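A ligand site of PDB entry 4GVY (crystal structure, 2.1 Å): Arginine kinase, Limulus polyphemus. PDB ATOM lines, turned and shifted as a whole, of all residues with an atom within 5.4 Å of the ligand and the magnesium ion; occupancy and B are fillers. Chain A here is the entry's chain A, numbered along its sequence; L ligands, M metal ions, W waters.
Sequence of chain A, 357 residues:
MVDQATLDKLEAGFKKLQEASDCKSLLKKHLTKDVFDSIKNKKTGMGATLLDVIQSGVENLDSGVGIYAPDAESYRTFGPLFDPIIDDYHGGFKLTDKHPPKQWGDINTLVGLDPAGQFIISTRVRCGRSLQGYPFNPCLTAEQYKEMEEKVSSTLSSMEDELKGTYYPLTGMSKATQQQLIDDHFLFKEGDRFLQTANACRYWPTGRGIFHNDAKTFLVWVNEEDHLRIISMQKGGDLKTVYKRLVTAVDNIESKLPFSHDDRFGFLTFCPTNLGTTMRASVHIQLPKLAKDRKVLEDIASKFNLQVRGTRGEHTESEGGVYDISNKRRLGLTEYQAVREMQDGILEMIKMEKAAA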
ATOM      1  N   SER A 122      28.219 -25.607  29.389  1.00  0.00           N
ATOM      2  CA  SER A 122      28.122 -24.960  28.087  1.00  0.00           C
ATOM      3  C   SER A 122      29.152 -23.840  27.969  1.00  0.00           C
ATOM      4  O   SER A 122      29.642 -23.302  28.967  1.00  0.00           O
ATOM      5  CB  SER A 122      26.724 -24.414  27.835  1.00  0.00           C
ATOM      6  OG  SER A 122      26.299 -23.568  28.886  1.00  0.00           O
ATOM      7  N   THR A 123      29.488 -23.500  26.723  1.00  0.00           N
ATOM      8  CA  THR A 123      30.506 -22.493  26.471  1.00  0.00           C
ATOM      9  C   THR A 123      29.959 -21.457  25.504  1.00  0.00           C
ATOM     10  O   THR A 123      29.252 -21.797  24.553  1.00  0.00           O
ATOM     11  CB  THR A 123      31.744 -23.171  25.852  1.00  0.00           C
ATOM     12  OG1 THR A 123      32.232 -24.171  26.759  1.00  0.00           O
ATOM     13  CG2 THR A 123      32.844 -22.145  25.594  1.00  0.00           C
ATOM     14  N   ARG A 124      30.304 -20.193  25.726  1.00  0.00           N
ATOM     15  CA  ARG A 124      29.701 -19.093  24.985  1.00  0.00           C
ATOM     16  C   ARG A 124      30.732 -17.993  24.762  1.00  0.00           C
ATOM     17  O   ARG A 124      31.473 -17.639  25.678  1.00  0.00           O
ATOM     18  CB  ARG A 124      28.525 -18.542  25.783  1.00  0.00           C
ATOM     19  CG  ARG A 124      27.799 -17.320  25.211  1.00  0.00           C
ATOM     20  CD  ARG A 124      26.579 -17.035  26.092  1.00  0.00           C
ATOM     21  NE  ARG A 124      25.738 -15.930  25.657  1.00  0.00           N
ATOM     22  CZ  ARG A 124      25.881 -14.666  26.045  1.00  0.00           C
ATOM     23  NH1 ARG A 124      26.910 -14.330  26.812  1.00  0.00           N
ATOM     24  NH2 ARG A 124      24.998 -13.751  25.684  1.00  0.00           N
ATOM     25  N   ARG A 126      30.676 -13.971  23.184  1.00  0.00           N
ATOM     26  CA  ARG A 126      29.971 -12.870  22.554  1.00  0.00           C
ATOM     27  C   ARG A 126      30.860 -11.667  22.289  1.00  0.00           C
ATOM     28  O   ARG A 126      31.848 -11.438  22.988  1.00  0.00           O
ATOM     29  CB  ARG A 126      28.690 -12.484  23.312  1.00  0.00           C
ATOM     30  CG  ARG A 126      28.852 -11.935  24.734  1.00  0.00           C
ATOM     31  CD  ARG A 126      29.261 -10.465  24.775  1.00  0.00           C
ATOM     32  NE  ARG A 126      29.062  -9.914  26.125  1.00  0.00           N
ATOM     33  CZ  ARG A 126      29.690  -8.841  26.605  1.00  0.00           C
ATOM     34  NH1 ARG A 126      29.407  -8.418  27.831  1.00  0.00           N
ATOM     35  NH2 ARG A 126      30.627  -8.232  25.900  1.00  0.00           N
ATOM     36  N   ILE A 182      14.645 -16.933  26.837  1.00  0.00           N
ATOM     37  CA  ILE A 182      15.405 -16.348  27.935  1.00  0.00           C
ATOM     38  C   ILE A 182      15.842 -17.432  28.916  1.00  0.00           C
ATOM     39  O   ILE A 182      16.984 -17.458  29.376  1.00  0.00           O
ATOM     40  CB  ILE A 182      14.602 -15.283  28.710  1.00  0.00           C
ATOM     41  CG1 ILE A 182      14.323 -14.065  27.823  1.00  0.00           C
ATOM     42  CG2 ILE A 182      15.333 -14.854  29.982  1.00  0.00           C
ATOM     43  CD1 ILE A 182      13.247 -13.133  28.394  1.00  0.00           C
ATOM     44  N   HIS A 185      18.772 -19.446  27.972  1.00  0.00           N
ATOM     45  CA  HIS A 185      20.021 -18.675  27.999  1.00  0.00           C
ATOM     46  C   HIS A 185      20.386 -18.088  26.647  1.00  0.00           C
ATOM     47  O   HIS A 185      21.520 -17.660  26.439  1.00  0.00           O
ATOM     48  CB  HIS A 185      21.194 -19.514  28.525  1.00  0.00           C
ATOM     49  CG  HIS A 185      20.906 -20.200  29.824  1.00  0.00           C
ATOM     50  ND1 HIS A 185      20.557 -19.507  30.965  1.00  0.00           N
ATOM     51  CD2 HIS A 185      20.889 -21.515  30.146  1.00  0.00           C
ATOM     52  CE1 HIS A 185      20.356 -20.369  31.951  1.00  0.00           C
ATOM     53  NE2 HIS A 185      20.546 -21.587  31.475  1.00  0.00           N
ATOM     54  N   PHE A 186      19.397 -18.015  25.754  1.00  0.00           N
ATOM     55  CA  PHE A 186      19.612 -17.512  24.406  1.00  0.00           C
ATOM     56  C   PHE A 186      19.269 -16.036  24.220  1.00  0.00           C
ATOM     57  O   PHE A 186      20.012 -15.299  23.581  1.00  0.00           O
ATOM     58  CB  PHE A 186      18.783 -18.336  23.409  1.00  0.00           C
ATOM     59  CG  PHE A 186      19.175 -19.789  23.361  1.00  0.00           C
ATOM     60  CD1 PHE A 186      18.216 -20.782  23.517  1.00  0.00           C
ATOM     61  CD2 PHE A 186      20.488 -20.165  23.143  1.00  0.00           C
ATOM     62  CE1 PHE A 186      18.569 -22.120  23.456  1.00  0.00           C
ATOM     63  CE2 PHE A 186      20.846 -21.506  23.089  1.00  0.00           C
ATOM     64  CZ  PHE A 186      19.884 -22.482  23.242  1.00  0.00           C
ATOM     65  N   LEU A 187      18.133 -15.612  24.765  1.00  0.00           N
ATOM     66  CA  LEU A 187      17.642 -14.265  24.534  1.00  0.00           C
ATOM     67  C   LEU A 187      17.920 -13.369  25.755  1.00  0.00           C
ATOM     68  O   LEU A 187      17.887 -13.835  26.902  1.00  0.00           O
ATOM     69  CB  LEU A 187      16.130 -14.287  24.261  1.00  0.00           C
ATOM     70  CG  LEU A 187      15.417 -12.952  24.055  1.00  0.00           C
ATOM     71  CD1 LEU A 187      16.013 -12.242  22.842  1.00  0.00           C
ATOM     72  CD2 LEU A 187      13.929 -13.154  23.860  1.00  0.00           C
ATOM     73  N   TRP A 221      21.758 -10.414  19.033  1.00  0.00           N
ATOM     74  CA  TRP A 221      20.777  -9.587  19.725  1.00  0.00           C
ATOM     75  C   TRP A 221      20.760  -8.237  19.051  1.00  0.00           C
ATOM     76  O   TRP A 221      21.807  -7.643  18.810  1.00  0.00           O
ATOM     77  CB  TRP A 221      21.201  -9.350  21.178  1.00  0.00           C
ATOM     78  CG  TRP A 221      21.151 -10.539  22.086  1.00  0.00           C
ATOM     79  CD1 TRP A 221      20.641 -11.772  21.795  1.00  0.00           C
ATOM     80  CD2 TRP A 221      21.595 -10.598  23.446  1.00  0.00           C
ATOM     81  NE1 TRP A 221      20.769 -12.596  22.884  1.00  0.00           N
ATOM     82  CE2 TRP A 221      21.357 -11.903  23.912  1.00  0.00           C
ATOM     83  CE3 TRP A 221      22.192  -9.673  24.308  1.00  0.00           C
ATOM     84  CZ2 TRP A 221      21.670 -12.305  25.213  1.00  0.00           C
ATOM     85  CZ3 TRP A 221      22.517 -10.074  25.600  1.00  0.00           C
ATOM     86  CH2 TRP A 221      22.259 -11.383  26.040  1.00  0.00           C
ATOM     87  N   GLU A 224      19.492  -4.418  22.246  1.00  0.00           N
ATOM     88  CA  GLU A 224      19.497  -4.503  23.709  1.00  0.00           C
ATOM     89  C   GLU A 224      20.491  -3.479  24.262  1.00  0.00           C
ATOM     90  O   GLU A 224      20.367  -2.289  23.974  1.00  0.00           O
ATOM     91  CB  GLU A 224      19.731  -5.932  24.224  1.00  0.00           C
ATOM     92  CG  GLU A 224      19.538  -6.053  25.751  1.00  0.00           C
ATOM     93  CD  GLU A 224      20.729  -6.638  26.482  1.00  0.00           C
ATOM     94  OE1 GLU A 224      21.883  -6.466  26.036  1.00  0.00           O
ATOM     95  OE2 GLU A 224      20.499  -7.271  27.540  1.00  0.00           O
ATOM     96  N   GLU A 225      21.506  -3.942  25.001  1.00  0.00           N
ATOM     97  CA  GLU A 225      22.474  -3.019  25.599  1.00  0.00           C
ATOM     98  C   GLU A 225      23.313  -2.355  24.508  1.00  0.00           C
ATOM     99  O   GLU A 225      23.589  -1.162  24.563  1.00  0.00           O
ATOM    100  CB  GLU A 225      23.406  -3.746  26.591  1.00  0.00           C
ATOM    101  CG  GLU A 225      24.502  -2.842  27.144  1.00  0.00           C
ATOM    102  CD  GLU A 225      25.359  -3.517  28.220  1.00  0.00           C
ATOM    103  OE1 GLU A 225      26.525  -3.108  28.361  1.00  0.00           O
ATOM    104  OE2 GLU A 225      24.891  -4.454  28.887  1.00  0.00           O
ATOM    105  N   ARG A 229      24.698  -7.638  19.640  1.00  0.00           N
ATOM    106  CA  ARG A 229      25.568  -8.570  20.318  1.00  0.00           C
ATOM    107  C   ARG A 229      25.576  -9.843  19.488  1.00  0.00           C
ATOM    108  O   ARG A 229      24.532 -10.435  19.249  1.00  0.00           O
ATOM    109  CB  ARG A 229      25.054  -8.891  21.732  1.00  0.00           C
ATOM    110  CG  ARG A 229      25.114  -7.709  22.698  1.00  0.00           C
ATOM    111  CD  ARG A 229      26.566  -7.393  23.068  1.00  0.00           C
ATOM    112  NE  ARG A 229      26.688  -6.370  24.105  1.00  0.00           N
ATOM    113  CZ  ARG A 229      26.421  -6.553  25.391  1.00  0.00           C
ATOM    114  NH1 ARG A 229      26.037  -7.746  25.834  1.00  0.00           N
ATOM    115  NH2 ARG A 229      26.550  -5.549  26.249  1.00  0.00           N
ATOM    116  N   MET A 233      27.518 -20.038  20.821  1.00  0.00           N
ATOM    117  CA  MET A 233      27.419 -20.839  22.038  1.00  0.00           C
ATOM    118  C   MET A 233      26.910 -22.234  21.715  1.00  0.00           C
ATOM    119  O   MET A 233      26.211 -22.442  20.721  1.00  0.00           O
ATOM    120  CB  MET A 233      26.491 -20.180  23.064  1.00  0.00           C
ATOM    121  CG  MET A 233      25.074 -19.903  22.558  1.00  0.00           C
ATOM    122  SD  MET A 233      24.114 -18.844  23.664  1.00  0.00           S
ATOM    123  CE  MET A 233      23.725 -19.950  25.011  1.00  0.00           C
ATOM    124  N   ASN A 274      32.858  -2.957  28.126  1.00  0.00           N
ATOM    125  CA  ASN A 274      32.746  -3.721  26.882  1.00  0.00           C
ATOM    126  C   ASN A 274      33.594  -3.180  25.728  1.00  0.00           C
ATOM    127  O   ASN A 274      33.473  -3.624  24.592  1.00  0.00           O
ATOM    128  CB  ASN A 274      31.276  -3.836  26.478  1.00  0.00           C
ATOM    129  CG  ASN A 274      30.536  -4.829  27.330  1.00  0.00           C
ATOM    130  OD1 ASN A 274      31.023  -5.918  27.624  1.00  0.00           O
ATOM    131  ND2 ASN A 274      29.361  -4.434  27.799  1.00  0.00           N
ATOM    132  N   ARG A 280      33.326 -11.309  25.646  1.00  0.00           N
ATOM    133  CA  ARG A 280      33.118 -12.028  26.893  1.00  0.00           C
ATOM    134  C   ARG A 280      32.966 -13.500  26.571  1.00  0.00           C
ATOM    135  O   ARG A 280      31.974 -13.916  25.971  1.00  0.00           O
ATOM    136  CB  ARG A 280      31.908 -11.505  27.680  1.00  0.00           C
ATOM    137  CG  ARG A 280      31.873 -12.022  29.106  1.00  0.00           C
ATOM    138  CD  ARG A 280      30.819 -11.328  29.964  1.00  0.00           C
ATOM    139  NE  ARG A 280      29.510 -11.965  29.922  1.00  0.00           N
ATOM    140  CZ  ARG A 280      29.200 -13.053  30.611  1.00  0.00           C
ATOM    141  NH1 ARG A 280      30.130 -13.643  31.364  1.00  0.00           N
ATOM    142  NH2 ARG A 280      27.971 -13.568  30.572  1.00  0.00           N
ATOM    143  N   SER A 282      32.697 -17.185  28.142  1.00  0.00           N
ATOM    144  CA  SER A 282      32.248 -17.701  29.430  1.00  0.00           C
ATOM    145  C   SER A 282      31.947 -19.179  29.365  1.00  0.00           C
ATOM    146  O   SER A 282      31.706 -19.741  28.303  1.00  0.00           O
ATOM    147  CB  SER A 282      30.979 -16.977  29.876  1.00  0.00           C
ATOM    148  OG  SER A 282      29.903 -17.299  29.017  1.00  0.00           O
ATOM    149  N   VAL A 283      31.977 -19.806  30.539  1.00  0.00           N
ATOM    150  CA  VAL A 283      31.421 -21.126  30.686  1.00  0.00           C
ATOM    151  C   VAL A 283      30.339 -21.107  31.746  1.00  0.00           C
ATOM    152  O   VAL A 283      30.383 -20.309  32.678  1.00  0.00           O
ATOM    153  CB  VAL A 283      32.509 -22.146  31.091  1.00  0.00           C
ATOM    154  CG1 VAL A 283      33.474 -22.383  29.921  1.00  0.00           C
ATOM    155  CG2 VAL A 283      33.244 -21.662  32.329  1.00  0.00           C
ATOM    156  N   HIS A 284      29.369 -21.991  31.590  1.00  0.00           N
ATOM    157  CA  HIS A 284      28.533 -22.372  32.708  1.00  0.00           C
ATOM    158  C   HIS A 284      29.149 -23.634  33.272  1.00  0.00           C
ATOM    159  O   HIS A 284      29.270 -24.641  32.562  1.00  0.00           O
ATOM    160  CB  HIS A 284      27.114 -22.641  32.223  1.00  0.00           C
ATOM    161  CG  HIS A 284      26.250 -21.417  32.202  1.00  0.00           C
ATOM    162  ND1 HIS A 284      24.873 -21.477  32.075  1.00  0.00           N
ATOM    163  CD2 HIS A 284      26.559 -20.105  32.337  1.00  0.00           C
ATOM    164  CE1 HIS A 284      24.380 -20.257  32.103  1.00  0.00           C
ATOM    165  NE2 HIS A 284      25.381 -19.401  32.262  1.00  0.00           N
ATOM    166  N   ARG A 309      29.487 -14.798  37.614  1.00  0.00           N
ATOM    167  CA  ARG A 309      28.102 -14.317  37.556  1.00  0.00           C
ATOM    168  C   ARG A 309      27.173 -15.487  37.855  1.00  0.00           C
ATOM    169  O   ARG A 309      27.574 -16.647  37.752  1.00  0.00           O
ATOM    170  CB  ARG A 309      27.803 -13.779  36.153  1.00  0.00           C
ATOM    171  CG  ARG A 309      28.616 -12.553  35.782  1.00  0.00           C
ATOM    172  CD  ARG A 309      28.372 -12.161  34.338  1.00  0.00           C
ATOM    173  NE  ARG A 309      29.204 -11.021  33.968  1.00  0.00           N
ATOM    174  CZ  ARG A 309      28.904 -10.131  33.036  1.00  0.00           C
ATOM    175  NH1 ARG A 309      27.803 -10.265  32.307  1.00  0.00           N
ATOM    176  NH2 ARG A 309      29.747  -9.126  32.802  1.00  0.00           N
ATOM    177  N   THR A 311      23.598 -17.898  37.275  1.00  0.00           N
ATOM    178  CA  THR A 311      23.190 -18.709  36.129  1.00  0.00           C
ATOM    179  C   THR A 311      22.387 -17.974  35.049  1.00  0.00           C
ATOM    180  O   THR A 311      22.519 -18.275  33.864  1.00  0.00           O
ATOM    181  CB  THR A 311      22.400 -19.943  36.587  1.00  0.00           C
ATOM    182  OG1 THR A 311      23.034 -20.499  37.748  1.00  0.00           O
ATOM    183  CG2 THR A 311      22.363 -20.995  35.482  1.00  0.00           C
ATOM    184  N   ARG A 312      21.584 -16.986  35.434  1.00  0.00           N
ATOM    185  CA  ARG A 312      20.779 -16.242  34.469  1.00  0.00           C
ATOM    186  C   ARG A 312      21.448 -14.942  34.003  1.00  0.00           C
ATOM    187  O   ARG A 312      20.826 -14.101  33.354  1.00  0.00           O
ATOM    188  CB  ARG A 312      19.377 -15.946  35.025  1.00  0.00           C
ATOM    189  CG  ARG A 312      18.521 -17.182  35.236  1.00  0.00           C
ATOM    190  CD  ARG A 312      17.165 -16.839  35.858  1.00  0.00           C
ATOM    191  NE  ARG A 312      16.239 -17.962  35.819  1.00  0.00           N
ATOM    192  CZ  ARG A 312      15.333 -18.175  34.869  1.00  0.00           C
ATOM    193  NH1 ARG A 312      15.231 -17.325  33.852  1.00  0.00           N
ATOM    194  NH2 ARG A 312      14.550 -19.236  34.919  1.00  0.00           N
ATOM    195  N   GLY A 313      22.730 -14.800  34.340  1.00  0.00           N
ATOM    196  CA  GLY A 313      23.543 -13.675  33.911  1.00  0.00           C
ATOM    197  C   GLY A 313      24.011 -12.825  35.092  1.00  0.00           C
ATOM    198  O   GLY A 313      23.846 -13.227  36.240  1.00  0.00           O
ATOM    199  N   GLU A 314      24.606 -11.668  34.802  1.00  0.00           N
ATOM    200  CA  GLU A 314      25.059 -10.760  35.857  1.00  0.00           C
ATOM    201  C   GLU A 314      23.935 -10.379  36.839  1.00  0.00           C
ATOM    202  O   GLU A 314      22.767 -10.386  36.468  1.00  0.00           O
ATOM    203  CB  GLU A 314      25.655  -9.492  35.246  1.00  0.00           C
ATOM    204  CG  GLU A 314      24.696  -8.780  34.310  1.00  0.00           C
ATOM    205  CD  GLU A 314      25.189  -7.404  33.927  1.00  0.00           C
ATOM    206  OE1 GLU A 314      26.141  -6.922  34.576  1.00  0.00           O
ATOM    207  OE2 GLU A 314      24.625  -6.803  32.988  1.00  0.00           O
ATOM    208  N   ASP A 324      28.419 -18.745  36.034  1.00  0.00           N
ATOM    209  CA  ASP A 324      28.917 -18.191  34.790  1.00  0.00           C
ATOM    210  C   ASP A 324      30.290 -17.594  35.118  1.00  0.00           C
ATOM    211  O   ASP A 324      30.398 -16.691  35.948  1.00  0.00           O
ATOM    212  CB  ASP A 324      27.916 -17.106  34.355  1.00  0.00           C
ATOM    213  CG  ASP A 324      28.414 -16.235  33.198  1.00  0.00           C
ATOM    214  OD1 ASP A 324      29.630 -16.121  32.975  1.00  0.00           O
ATOM    215  OD2 ASP A 324      27.543 -15.634  32.524  1.00  0.00           O
HETATM  216  P1  LIG L   1      26.279 -10.459  28.346  1.00  0.00           P
HETATM  217  O1  LIG L   1      25.184  -9.437  28.152  1.00  0.00           O
HETATM  218  O2  LIG L   1      26.371 -11.530  27.290  1.00  0.00           O
HETATM  219  O3  LIG L   1      27.562  -9.841  28.838  1.00  0.00           O
HETATM  220  P2  LIG L   1      24.803 -11.457  30.714  1.00  0.00           P
HETATM  221  O4  LIG L   1      23.689 -10.465  30.549  1.00  0.00           O
HETATM  222  O5  LIG L   1      25.251 -11.940  32.061  1.00  0.00           O
HETATM  223  O6  LIG L   1      25.800 -11.625  29.548  1.00  0.00           O
HETATM  224  O7  LIG L   1      23.801 -12.890  30.342  1.00  0.00           O
HETATM  225  C1  LIG L   1      23.258 -13.025  29.141  1.00  0.00           C
HETATM  226  C2  LIG L   1      22.677 -14.460  28.929  1.00  0.00           C
HETATM  227  O8  LIG L   1      23.741 -15.352  28.591  1.00  0.00           O
HETATM  228  C3  LIG L   1      22.057 -15.030  30.210  1.00  0.00           C
HETATM  229  O9  LIG L   1      20.890 -15.742  29.937  1.00  0.00           O
HETATM  230  C4  LIG L   1      23.094 -16.091  30.695  1.00  0.00           C
HETATM  231  O10 LIG L   1      22.465 -17.225  31.187  1.00  0.00           O
HETATM  232  C5  LIG L   1      23.660 -16.496  29.326  1.00  0.00           C
HETATM  233  N1  LIG L   1      24.997 -17.164  29.356  1.00  0.00           N
HETATM  234  C6  LIG L   1      26.203 -16.537  29.738  1.00  0.00           C
HETATM  235  N2  LIG L   1      27.265 -17.384  29.681  1.00  0.00           N
HETATM  236  C7  LIG L   1      26.712 -18.594  29.244  1.00  0.00           C
HETATM  237  C8  LIG L   1      27.285 -19.862  28.979  1.00  0.00           C
HETATM  238  N3  LIG L   1      28.635 -20.086  29.139  1.00  0.00           N
HETATM  239  N4  LIG L   1      26.508 -20.896  28.543  1.00  0.00           N
HETATM  240  C9  LIG L   1      25.164 -20.632  28.395  1.00  0.00           C
HETATM  241  N5  LIG L   1      24.490 -19.482  28.609  1.00  0.00           N
HETATM  242  C10 LIG L   1      25.306 -18.458  29.036  1.00  0.00           C
HETATM  243 MG    MG M   1      23.824  -8.596  29.352  1.00  0.00          MG
HETATM  244  O   HOH W   1      28.538  -7.334  30.882  1.00  0.00           O
HETATM  245  O   HOH W   2      23.871  -6.873  28.230  1.00  0.00           O
HETATM  246  O   HOH W   3      19.255 -13.625  29.358  1.00  0.00           O
HETATM  247  O   HOH W   4      25.769 -10.325  24.667  1.00  0.00           O
HETATM  248  O   HOH W   5      22.914  -7.576  30.932  1.00  0.00           O
HETATM  249  O   HOH W   6      21.957  -9.101  28.665  1.00  0.00           O
HETATM  250  O   HOH W   7      25.533  -8.043  30.314  1.00  0.00           O
HETATM  251  O   HOH W   8      18.801 -16.973  31.394  1.00  0.00           O
HETATM  252  O   HOH W   9      18.598 -14.301  32.045  1.00  0.00           O
HETATM  253  O   HOH W  10      25.104 -16.566  33.047  1.00  0.00           O
HETATM  254  O   HOH W  11      21.346 -10.210  31.888  1.00  0.00           O
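NH1 of Arg 126 is in salt-bridge range of O3 of the ligand (2.5 Å). The backbone carbonyl oxygen of Ser 122 sits at hydrogen-bond distance from a nitrogen (N3) of the ligand (3.4 Å). The side-chain hydroxyl of Ser 122 is in hydrogen-bond range of a nitrogen (N4) of the ligand, at 2.7 Å. The backbone carbonyl oxygen of Ser 282 sits at hydrogen-bond distance from a nitrogen (N3) of the ligand. OG of Ser 282 sits at hydrogen-bond distance from N2 of the ligand, 2.7 Å away. An oxygen (O5) of the ligand sits at hydrogen-bond distance from the backbone NH (N) of Glu 314, at 2.8 Å. An oxygen (O10) of the ligand lies within hydrogen-bond range of the backbone carbonyl oxygen (O) of Thr 311 (2.9 Å). O2 of the ligand lies within salt-bridge range of NH1 of Arg 124 (2.9 Å). An oxygen (O10) of the ligand is in hydrogen-bond range of a ring nitrogen (ND1) of His 185 (3.0 Å). The guanidinium group (NH1) of Arg 229 is in salt-bridge range of an oxygen (O3) of the ligand (3.97 Å). NH1 of Arg 309 lies within salt-bridge range of O5 of the ligand, 3.1 Å away. NE of Arg 280 is in salt-bridge range of O3 of the ligand, at 3.1 Å.
The backbone carbonyl oxygen of Arg 126 lies within hydrogen-bond range of the backbone NH of Arg 280, at 3.0 Å. The side-chain amide oxygen (OD1) of Asn 274 lies within hydrogen-bond range of the guanidinium group (NH2) of Arg 126, 2.9 Å away. The backbone NH of His 284 is in hydrogen-bond range of the backbone carbonyl oxygen of Ser 122 (2.9 Å). The backbone carbonyl oxygen (O) of Arg 124 is in hydrogen-bond range of the backbone NH (N) of Ser 282, 2.8 Å away. The backbone carbonyl oxygen of Thr 311 lies close to a ring nitrogen (NE2) of His 284 (3.5 Å). OE1 of Glu 225 is in salt-bridge range of NH2 of Arg 229 (3.2 Å). The guanidinium group (NH2) of Arg 229 sits close to the side-chain amide nitrogen (ND2) of Asn 274 (3.4 Å). The indole nitrogen (NE1) of Trp 221 sits at hydrogen-bond distance from the backbone carbonyl oxygen (O) of Phe 186 (2.9 Å).
N3 of the ligand lies close to N of His 284 (3.2 Å). The side-chain carboxylate (OD2) of Asp 324 lies close to a nitrogen (N2) of the ligand, 3.3 Å away. Trp 221 touches the ligand (CH2 to C1, 3.6 Å). Met 233 touches the ligand (CE to N5, 3.7 Å). Val 283 touches the ligand (C to N3, 3.3 Å). O of Arg 312 touches C3 of the ligand, at 3.5 Å. Gly 313 touches the ligand. Along chain A the residues within 4 Å of the ligand span positions 122 to 324.
No residue comes within 4 Å of the magnesium ion. The nearest printed residue that does not touch the magnesium ion is Glu 224 (4.01 Å).
The magnesium ion is bound by an oxygen (O1) of the ligand, water W7, water W6, water W2, water W5 and an oxygen (O4) of the ligand. The magnesium ion has six donor atoms within binding distance.
Water W7 lies within hydrogen-bond range of the side-chain carboxylate (OE2) of Glu 314 and an oxygen (O3) of the ligand. Water W8 lies within hydrogen-bond range of O of Ile 182 (2.8 Å), O9 of the ligand (2.8 Å) and ND1 of His 185 (3.1 Å). Water W4 bridges NH1 of Arg 229 and O2 of the ligand. Water W10 lies within hydrogen-bond range of the side-chain carboxylate (OD2) of Asp 324, a ring nitrogen (NE2) of His 284, the backbone carbonyl oxygen (O) of Thr 311, the backbone NH (N) of Gly 313 and an oxygen (O10) of the ligand. Water W1 lies within hydrogen-bond range of NH2 of Arg 309 (2.9 Å), NH1 of Arg 126 (3.4 Å) and O3 of the ligand (3.4 Å). Water W9 lies within hydrogen-bond range of the backbone carbonyl oxygen (O) of Arg 312 (2.6 Å) and an oxygen (O9) of the ligand (3.4 Å).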
